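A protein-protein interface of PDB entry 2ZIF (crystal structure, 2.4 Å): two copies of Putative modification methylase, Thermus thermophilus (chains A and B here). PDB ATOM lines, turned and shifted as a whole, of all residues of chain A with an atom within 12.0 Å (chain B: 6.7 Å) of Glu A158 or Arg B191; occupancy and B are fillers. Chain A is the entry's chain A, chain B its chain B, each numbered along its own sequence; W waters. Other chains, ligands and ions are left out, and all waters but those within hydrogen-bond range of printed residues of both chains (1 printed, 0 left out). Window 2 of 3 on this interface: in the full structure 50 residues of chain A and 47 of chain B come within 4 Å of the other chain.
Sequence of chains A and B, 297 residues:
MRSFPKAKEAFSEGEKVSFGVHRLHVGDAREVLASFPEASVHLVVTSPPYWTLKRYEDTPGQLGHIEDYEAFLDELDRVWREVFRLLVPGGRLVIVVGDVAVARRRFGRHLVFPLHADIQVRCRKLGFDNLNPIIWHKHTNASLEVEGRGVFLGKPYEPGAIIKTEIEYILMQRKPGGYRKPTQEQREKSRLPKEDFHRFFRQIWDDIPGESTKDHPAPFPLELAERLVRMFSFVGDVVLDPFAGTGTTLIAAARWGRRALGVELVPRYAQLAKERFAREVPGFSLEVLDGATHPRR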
ATOM      1  N   PRO A 156      -9.899 -30.050  16.414  1.00  0.00           N
ATOM      2  CA  PRO A 156     -10.653 -29.314  17.435  1.00  0.00           C
ATOM      3  C   PRO A 156     -10.278 -29.768  18.846  1.00  0.00           C
ATOM      4  O   PRO A 156     -11.148 -29.951  19.699  1.00  0.00           O
ATOM      5  CB  PRO A 156     -12.095 -29.652  17.088  1.00  0.00           C
ATOM      6  CG  PRO A 156     -11.980 -31.093  16.670  1.00  0.00           C
ATOM      7  CD  PRO A 156     -10.752 -31.066  15.766  1.00  0.00           C
ATOM      8  N   TYR A 157      -8.982 -29.935  19.081  1.00  0.00           N
ATOM      9  CA  TYR A 157      -8.455 -30.384  20.371  1.00  0.00           C
ATOM     10  C   TYR A 157      -8.752 -29.417  21.511  1.00  0.00           C
ATOM     11  O   TYR A 157      -7.844 -28.850  22.115  1.00  0.00           O
ATOM     12  CB  TYR A 157      -6.948 -30.593  20.250  1.00  0.00           C
ATOM     13  CG  TYR A 157      -6.565 -31.419  19.044  1.00  0.00           C
ATOM     14  CD1 TYR A 157      -7.126 -32.677  18.832  1.00  0.00           C
ATOM     15  CD2 TYR A 157      -5.653 -30.941  18.107  1.00  0.00           C
ATOM     16  CE1 TYR A 157      -6.791 -33.439  17.714  1.00  0.00           C
ATOM     17  CE2 TYR A 157      -5.308 -31.697  16.982  1.00  0.00           C
ATOM     18  CZ  TYR A 157      -5.884 -32.943  16.794  1.00  0.00           C
ATOM     19  OH  TYR A 157      -5.563 -33.693  15.685  1.00  0.00           O
ATOM     20  N   GLU A 158     -10.035 -29.248  21.808  1.00  0.00           N
ATOM     21  CA  GLU A 158     -10.464 -28.345  22.863  1.00  0.00           C
ATOM     22  C   GLU A 158     -11.103 -29.075  24.042  1.00  0.00           C
ATOM     23  O   GLU A 158     -11.707 -30.131  23.881  1.00  0.00           O
ATOM     24  CB  GLU A 158     -11.458 -27.329  22.292  1.00  0.00           C
ATOM     25  CG  GLU A 158     -10.815 -26.282  21.406  1.00  0.00           C
ATOM     26  CD  GLU A 158     -11.829 -25.410  20.694  1.00  0.00           C
ATOM     27  OE1 GLU A 158     -12.736 -24.873  21.365  1.00  0.00           O
ATOM     28  OE2 GLU A 158     -11.709 -25.260  19.461  1.00  0.00           O
ATOM     29  N   PRO A 159     -10.978 -28.506  25.248  1.00  0.00           N
ATOM     30  CA  PRO A 159     -11.545 -29.091  26.461  1.00  0.00           C
ATOM     31  C   PRO A 159     -12.980 -29.585  26.254  1.00  0.00           C
ATOM     32  O   PRO A 159     -13.707 -29.046  25.427  1.00  0.00           O
ATOM     33  CB  PRO A 159     -11.475 -27.935  27.451  1.00  0.00           C
ATOM     34  CG  PRO A 159     -10.203 -27.255  27.052  1.00  0.00           C
ATOM     35  CD  PRO A 159     -10.283 -27.239  25.549  1.00  0.00           C
ATOM     36  N   GLY A 160     -13.366 -30.617  27.002  1.00  0.00           N
ATOM     37  CA  GLY A 160     -14.711 -31.161  26.915  1.00  0.00           C
ATOM     38  C   GLY A 160     -14.932 -32.363  26.009  1.00  0.00           C
ATOM     39  O   GLY A 160     -16.019 -32.940  26.007  1.00  0.00           O
ATOM     40  N   ALA A 161     -13.923 -32.753  25.236  1.00  0.00           N
ATOM     41  CA  ALA A 161     -14.075 -33.893  24.335  1.00  0.00           C
ATOM     42  C   ALA A 161     -14.538 -35.156  25.064  1.00  0.00           C
ATOM     43  O   ALA A 161     -14.239 -35.354  26.245  1.00  0.00           O
ATOM     44  CB  ALA A 161     -12.763 -34.163  23.613  1.00  0.00           C
ATOM     45  N   ILE A 162     -15.284 -35.997  24.355  1.00  0.00           N
ATOM     46  CA  ILE A 162     -15.769 -37.254  24.917  1.00  0.00           C
ATOM     47  C   ILE A 162     -14.684 -38.309  24.737  1.00  0.00           C
ATOM     48  O   ILE A 162     -14.083 -38.412  23.667  1.00  0.00           O
ATOM     49  CB  ILE A 162     -17.045 -37.738  24.194  1.00  0.00           C
ATOM     50  CG1 ILE A 162     -18.153 -36.700  24.358  1.00  0.00           C
ATOM     51  CG2 ILE A 162     -17.487 -39.089  24.747  1.00  0.00           C
ATOM     52  CD1 ILE A 162     -18.445 -36.326  25.815  1.00  0.00           C
ATOM     53  N   ILE A 163     -14.418 -39.091  25.777  1.00  0.00           N
ATOM     54  CA  ILE A 163     -13.404 -40.126  25.651  1.00  0.00           C
ATOM     55  C   ILE A 163     -14.106 -41.406  25.219  1.00  0.00           C
ATOM     56  O   ILE A 163     -15.078 -41.819  25.835  1.00  0.00           O
ATOM     57  CB  ILE A 163     -12.642 -40.358  26.989  1.00  0.00           C
ATOM     58  CG1 ILE A 163     -12.156 -39.016  27.559  1.00  0.00           C
ATOM     59  CG2 ILE A 163     -11.439 -41.276  26.748  1.00  0.00           C
ATOM     60  CD1 ILE A 163     -11.282 -39.122  28.796  1.00  0.00           C
ATOM     61  N   PRO B 182     -17.536 -20.513  25.704  1.00  0.00           N
ATOM     62  CA  PRO B 182     -16.292 -19.795  26.008  1.00  0.00           C
ATOM     63  C   PRO B 182     -15.968 -18.715  24.975  1.00  0.00           C
ATOM     64  O   PRO B 182     -16.411 -18.794  23.829  1.00  0.00           O
ATOM     65  CB  PRO B 182     -15.266 -20.910  25.987  1.00  0.00           C
ATOM     66  CG  PRO B 182     -15.724 -21.699  24.797  1.00  0.00           C
ATOM     67  CD  PRO B 182     -17.240 -21.758  24.968  1.00  0.00           C
ATOM     68  N   GLN B 184     -13.432 -16.415  22.454  1.00  0.00           N
ATOM     69  CA  GLN B 184     -12.479 -16.861  21.446  1.00  0.00           C
ATOM     70  C   GLN B 184     -11.086 -16.987  22.052  1.00  0.00           C
ATOM     71  O   GLN B 184     -10.309 -17.877  21.687  1.00  0.00           O
ATOM     72  CB  GLN B 184     -12.446 -15.871  20.276  1.00  0.00           C
ATOM     73  CG  GLN B 184     -11.578 -16.310  19.106  1.00  0.00           C
ATOM     74  CD  GLN B 184     -12.118 -17.551  18.427  1.00  0.00           C
ATOM     75  OE1 GLN B 184     -11.456 -18.146  17.576  1.00  0.00           O
ATOM     76  NE2 GLN B 184     -13.333 -17.949  18.799  1.00  0.00           N
ATOM     77  N   GLN B 186     -10.530 -17.683  25.136  1.00  0.00           N
ATOM     78  CA  GLN B 186     -10.544 -18.824  26.039  1.00  0.00           C
ATOM     79  C   GLN B 186     -10.250 -20.092  25.245  1.00  0.00           C
ATOM     80  O   GLN B 186      -9.515 -20.964  25.705  1.00  0.00           O
ATOM     81  CB  GLN B 186     -11.892 -18.953  26.759  1.00  0.00           C
ATOM     82  CG  GLN B 186     -12.055 -18.029  27.967  1.00  0.00           C
ATOM     83  CD  GLN B 186     -13.376 -18.241  28.689  1.00  0.00           C
ATOM     84  OE1 GLN B 186     -14.434 -18.292  28.063  1.00  0.00           O
ATOM     85  NE2 GLN B 186     -13.323 -18.361  30.012  1.00  0.00           N
ATOM     86  N   ARG B 187     -10.813 -20.185  24.047  1.00  0.00           N
ATOM     87  CA  ARG B 187     -10.583 -21.352  23.216  1.00  0.00           C
ATOM     88  C   ARG B 187      -9.128 -21.369  22.759  1.00  0.00           C
ATOM     89  O   ARG B 187      -8.448 -22.389  22.885  1.00  0.00           O
ATOM     90  CB  ARG B 187     -11.539 -21.349  22.017  1.00  0.00           C
ATOM     91  CG  ARG B 187     -12.993 -21.535  22.432  1.00  0.00           C
ATOM     92  CD  ARG B 187     -14.019 -21.318  21.311  1.00  0.00           C
ATOM     93  NE  ARG B 187     -14.018 -22.365  20.291  1.00  0.00           N
ATOM     94  CZ  ARG B 187     -13.158 -22.426  19.278  1.00  0.00           C
ATOM     95  NH1 ARG B 187     -13.234 -23.417  18.400  1.00  0.00           N
ATOM     96  NH2 ARG B 187     -12.227 -21.494  19.134  1.00  0.00           N
ATOM     97  N   GLU B 188      -8.641 -20.238  22.259  1.00  0.00           N
ATOM     98  CA  GLU B 188      -7.261 -20.150  21.790  1.00  0.00           C
ATOM     99  C   GLU B 188      -6.258 -20.481  22.879  1.00  0.00           C
ATOM    100  O   GLU B 188      -5.240 -21.113  22.613  1.00  0.00           O
ATOM    101  CB  GLU B 188      -6.939 -18.748  21.259  1.00  0.00           C
ATOM    102  CG  GLU B 188      -7.578 -18.388  19.933  1.00  0.00           C
ATOM    103  CD  GLU B 188      -7.241 -16.966  19.510  1.00  0.00           C
ATOM    104  OE1 GLU B 188      -7.409 -16.035  20.340  1.00  0.00           O
ATOM    105  OE2 GLU B 188      -6.814 -16.775  18.349  1.00  0.00           O
ATOM    106  N   LYS B 189      -6.541 -20.041  24.100  1.00  0.00           N
ATOM    107  CA  LYS B 189      -5.628 -20.272  25.215  1.00  0.00           C
ATOM    108  C   LYS B 189      -5.833 -21.574  25.989  1.00  0.00           C
ATOM    109  O   LYS B 189      -5.005 -21.941  26.820  1.00  0.00           O
ATOM    110  CB  LYS B 189      -5.673 -19.087  26.178  1.00  0.00           C
ATOM    111  CG  LYS B 189      -5.120 -17.806  25.580  1.00  0.00           C
ATOM    112  CD  LYS B 189      -5.096 -16.697  26.616  1.00  0.00           C
ATOM    113  CE  LYS B 189      -4.591 -15.387  26.036  1.00  0.00           C
ATOM    114  NZ  LYS B 189      -4.571 -14.332  27.092  1.00  0.00           N
ATOM    115  N   SER B 190      -6.927 -22.273  25.719  1.00  0.00           N
ATOM    116  CA  SER B 190      -7.192 -23.531  26.395  1.00  0.00           C
ATOM    117  C   SER B 190      -6.967 -24.686  25.437  1.00  0.00           C
ATOM    118  O   SER B 190      -6.833 -25.831  25.866  1.00  0.00           O
ATOM    119  CB  SER B 190      -8.626 -23.571  26.919  1.00  0.00           C
ATOM    120  OG  SER B 190      -8.857 -22.490  27.797  1.00  0.00           O
ATOM    121  N   ARG B 191      -6.940 -24.384  24.141  1.00  0.00           N
ATOM    122  CA  ARG B 191      -6.725 -25.405  23.127  1.00  0.00           C
ATOM    123  C   ARG B 191      -5.480 -26.219  23.487  1.00  0.00           C
ATOM    124  O   ARG B 191      -4.408 -25.661  23.747  1.00  0.00           O
ATOM    125  CB  ARG B 191      -6.556 -24.758  21.743  1.00  0.00           C
ATOM    126  CG  ARG B 191      -6.140 -25.738  20.641  1.00  0.00           C
ATOM    127  CD  ARG B 191      -6.009 -25.072  19.277  1.00  0.00           C
ATOM    128  NE  ARG B 191      -7.299 -24.606  18.759  1.00  0.00           N
ATOM    129  CZ  ARG B 191      -7.576 -23.341  18.452  1.00  0.00           C
ATOM    130  NH1 ARG B 191      -6.656 -22.392  18.608  1.00  0.00           N
ATOM    131  NH2 ARG B 191      -8.777 -23.024  17.988  1.00  0.00           N
ATOM    132  N   LEU B 192      -5.628 -27.539  23.512  1.00  0.00           N
ATOM    133  CA  LEU B 192      -4.511 -28.403  23.849  1.00  0.00           C
ATOM    134  C   LEU B 192      -3.741 -28.841  22.613  1.00  0.00           C
ATOM    135  O   LEU B 192      -4.332 -29.147  21.581  1.00  0.00           O
ATOM    136  CB  LEU B 192      -4.997 -29.651  24.597  1.00  0.00           C
ATOM    137  CG  LEU B 192      -5.633 -29.494  25.985  1.00  0.00           C
ATOM    138  CD1 LEU B 192      -7.121 -29.166  25.864  1.00  0.00           C
ATOM    139  CD2 LEU B 192      -5.467 -30.794  26.747  1.00  0.00           C
ATOM    140  N   PRO B 193      -2.401 -28.867  22.705  1.00  0.00           N
ATOM    141  CA  PRO B 193      -1.555 -29.287  21.587  1.00  0.00           C
ATOM    142  C   PRO B 193      -1.973 -30.717  21.246  1.00  0.00           C
ATOM    143  O   PRO B 193      -2.436 -31.456  22.111  1.00  0.00           O
ATOM    144  CB  PRO B 193      -0.148 -29.242  22.181  1.00  0.00           C
ATOM    145  CG  PRO B 193      -0.257 -28.207  23.249  1.00  0.00           C
ATOM    146  CD  PRO B 193      -1.587 -28.504  23.875  1.00  0.00           C
ATOM    147  N   PHE B 197      -3.341 -33.669  23.892  1.00  0.00           N
ATOM    148  CA  PHE B 197      -4.722 -34.100  23.733  1.00  0.00           C
ATOM    149  C   PHE B 197      -4.856 -35.630  23.690  1.00  0.00           C
ATOM    150  O   PHE B 197      -5.684 -36.203  24.390  1.00  0.00           O
ATOM    151  CB  PHE B 197      -5.314 -33.502  22.459  1.00  0.00           C
ATOM    152  CG  PHE B 197      -6.743 -33.865  22.243  1.00  0.00           C
ATOM    153  CD1 PHE B 197      -7.760 -33.105  22.817  1.00  0.00           C
ATOM    154  CD2 PHE B 197      -7.078 -35.000  21.517  1.00  0.00           C
ATOM    155  CE1 PHE B 197      -9.091 -33.474  22.673  1.00  0.00           C
ATOM    156  CE2 PHE B 197      -8.410 -35.384  21.367  1.00  0.00           C
ATOM    157  CZ  PHE B 197      -9.419 -34.622  21.946  1.00  0.00           C
ATOM    158  N   PHE B 201      -6.807 -37.486  26.616  1.00  0.00           N
ATOM    159  CA  PHE B 201      -8.107 -38.051  26.290  1.00  0.00           C
ATOM    160  C   PHE B 201      -8.121 -39.528  25.910  1.00  0.00           C
ATOM    161  O   PHE B 201      -8.382 -39.891  24.768  1.00  0.00           O
ATOM    162  CB  PHE B 201      -8.788 -37.219  25.197  1.00  0.00           C
ATOM    163  CG  PHE B 201      -9.318 -35.904  25.692  1.00  0.00           C
ATOM    164  CD1 PHE B 201      -8.497 -34.784  25.758  1.00  0.00           C
ATOM    165  CD2 PHE B 201     -10.619 -35.811  26.185  1.00  0.00           C
ATOM    166  CE1 PHE B 201      -8.963 -33.593  26.318  1.00  0.00           C
ATOM    167  CE2 PHE B 201     -11.089 -34.625  26.745  1.00  0.00           C
ATOM    168  CZ  PHE B 201     -10.262 -33.520  26.811  1.00  0.00           C
ATOM    169  N   ARG B 230      -6.926 -28.887  32.631  1.00  0.00           N
ATOM    170  CA  ARG B 230      -6.758 -28.514  31.227  1.00  0.00           C
ATOM    171  C   ARG B 230      -7.799 -29.155  30.325  1.00  0.00           C
ATOM    172  O   ARG B 230      -8.194 -28.584  29.311  1.00  0.00           O
ATOM    173  CB  ARG B 230      -5.372 -28.914  30.717  1.00  0.00           C
ATOM    174  CG  ARG B 230      -4.234 -28.138  31.334  1.00  0.00           C
ATOM    175  CD  ARG B 230      -2.905 -28.711  30.894  1.00  0.00           C
ATOM    176  NE  ARG B 230      -2.612 -28.405  29.498  1.00  0.00           N
ATOM    177  CZ  ARG B 230      -1.561 -28.876  28.838  1.00  0.00           C
ATOM    178  NH1 ARG B 230      -0.697 -29.686  29.448  1.00  0.00           N
ATOM    179  NH2 ARG B 230      -1.369 -28.536  27.572  1.00  0.00           N
ATOM    180  N   MET B 231      -8.230 -30.353  30.703  1.00  0.00           N
ATOM    181  CA  MET B 231      -9.209 -31.091  29.925  1.00  0.00           C
ATOM    182  C   MET B 231     -10.649 -30.623  30.090  1.00  0.00           C
ATOM    183  O   MET B 231     -11.411 -30.601  29.125  1.00  0.00           O
ATOM    184  CB  MET B 231      -9.164 -32.581  30.287  1.00  0.00           C
ATOM    185  CG  MET B 231      -7.910 -33.329  29.869  1.00  0.00           C
ATOM    186  SD  MET B 231      -7.907 -35.003  30.601  1.00  0.00           S
ATOM    187  CE  MET B 231      -8.962 -35.906  29.443  1.00  0.00           C
ATOM    188  N   PHE B 234     -11.816 -23.962  31.160  1.00  0.00           N
ATOM    189  CA  PHE B 234     -11.143 -22.997  30.299  1.00  0.00           C
ATOM    190  C   PHE B 234     -10.381 -22.000  31.157  1.00  0.00           C
ATOM    191  O   PHE B 234     -10.724 -21.790  32.324  1.00  0.00           O
ATOM    192  CB  PHE B 234     -12.165 -22.234  29.453  1.00  0.00           C
ATOM    193  CG  PHE B 234     -12.778 -23.048  28.356  1.00  0.00           C
ATOM    194  CD1 PHE B 234     -12.071 -23.295  27.179  1.00  0.00           C
ATOM    195  CD2 PHE B 234     -14.066 -23.567  28.491  1.00  0.00           C
ATOM    196  CE1 PHE B 234     -12.639 -24.045  26.153  1.00  0.00           C
ATOM    197  CE2 PHE B 234     -14.640 -24.321  27.467  1.00  0.00           C
ATOM    198  CZ  PHE B 234     -13.928 -24.558  26.299  1.00  0.00           C
ATOM    199  N   ARG B 258      -6.624 -20.683  35.826  1.00  0.00           N
ATOM    200  CA  ARG B 258      -8.020 -20.864  36.224  1.00  0.00           C
ATOM    201  C   ARG B 258      -8.175 -20.283  37.630  1.00  0.00           C
ATOM    202  O   ARG B 258      -7.204 -20.220  38.391  1.00  0.00           O
ATOM    203  CB  ARG B 258      -8.399 -22.351  36.268  1.00  0.00           C
ATOM    204  CG  ARG B 258      -8.879 -22.969  34.952  1.00  0.00           C
ATOM    205  CD  ARG B 258      -7.755 -23.141  33.934  1.00  0.00           C
ATOM    206  NE  ARG B 258      -8.215 -23.888  32.766  1.00  0.00           N
ATOM    207  CZ  ARG B 258      -7.493 -24.091  31.671  1.00  0.00           C
ATOM    208  NH1 ARG B 258      -6.263 -23.594  31.587  1.00  0.00           N
ATOM    209  NH2 ARG B 258      -7.992 -24.801  30.665  1.00  0.00           N
HETATM  210  O   HOH W   1      -9.812 -25.670  17.811  1.00  0.00           O
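The backbone NH of Gly A160 lies within hydrogen-bond range of the backbone carbonyl oxygen of Met B231 (2.9 Å).
OE2 of Glu A158 is in salt-bridge range of NH1 of Arg B187 (2.6 Å).
The backbone carbonyl oxygen of Tyr A157 is in hydrogen-bond range of the backbone NH of Leu B192.
The side-chain carboxylate of Glu A158 is in salt-bridge range of the guanidinium group of Arg B191, 3.97 Å away.
The backbone carbonyl oxygen (O) of Gln B186 lies within hydrogen-bond range of the side-chain hydroxyl (OG) of Ser B190 (2.7 Å).
Arg B191 touches Tyr A157 (CA to O, 3.8 Å).
Phe B197 touches Tyr A157 (CD2 to CD1, 3.6 Å).
CD of Pro A159 touches O of Ser B190, 3.7 Å away.
CD of Pro A159 touches CD1 of Leu B192 (3.7 Å).
Pro A159 touches Arg B230.
CA of Pro A159 touches O of Met B231 (3.1 Å).
Ala A161 touches Phe B197.
Ala A161 touches Phe B201.
Phe B201 touches Ile A163.
Of the printed residues of chain B, Glu A158 touches Arg B187 (2.6 Å) and Arg B191 (3.97 Å).
Printed residues of chain A within 4 Å of Arg B191: Tyr A157 (3.8 Å) and Glu A158 (3.97 Å).
No residue of chain A comes within 4 Å of Pro B182.
No residue of chain A comes within 4 Å of Glu B188.
Leu B192 touches two residues of chain A.
No residue of chain A comes within 4 Å of Pro B193.
Of the printed residues of chain B, Ile A163 touches Phe B201 (3.8 Å).
Of the printed residues of chain B, Gly A160 touches Met B231.
The nearest residue of chain B that does not touch Glu A158 is Leu B192 (4.4 Å).
The nearest residue of chain A that does not touch Arg B191 is Pro A159 (4.6 Å).
The nearest printed residue of chain B that does not touch Tyr A157 is Pro B193 (4.8 Å).
Of the 16 printed residues of chain B, 8 touch a printed residue of chain A.
Printed residues of chain B that touch a printed residue of chain A: Arg B187, Ser B190, Arg B191, Leu B192, Phe B197, Phe B201, Arg B230 and Met B231.
Hydrophobic or aromatic side chains of chain B within 4 Å of the printed part of chain A: Leu B192, Phe B197 and Phe B201.
Of the 8 printed residues of chain A, 6 touch a printed residue of chain B.
Along chain A the printed residues that touch a printed residue of chain B span positions 157 to 163.
Among the printed residues, 13 pairs touch across the chains.
No position is printed for both chains.
Water W1 lies within hydrogen-bond range of the side-chain carboxylate of Glu A158 (2.5 Å) and the guanidinium group of Arg B191 (2.8 Å).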
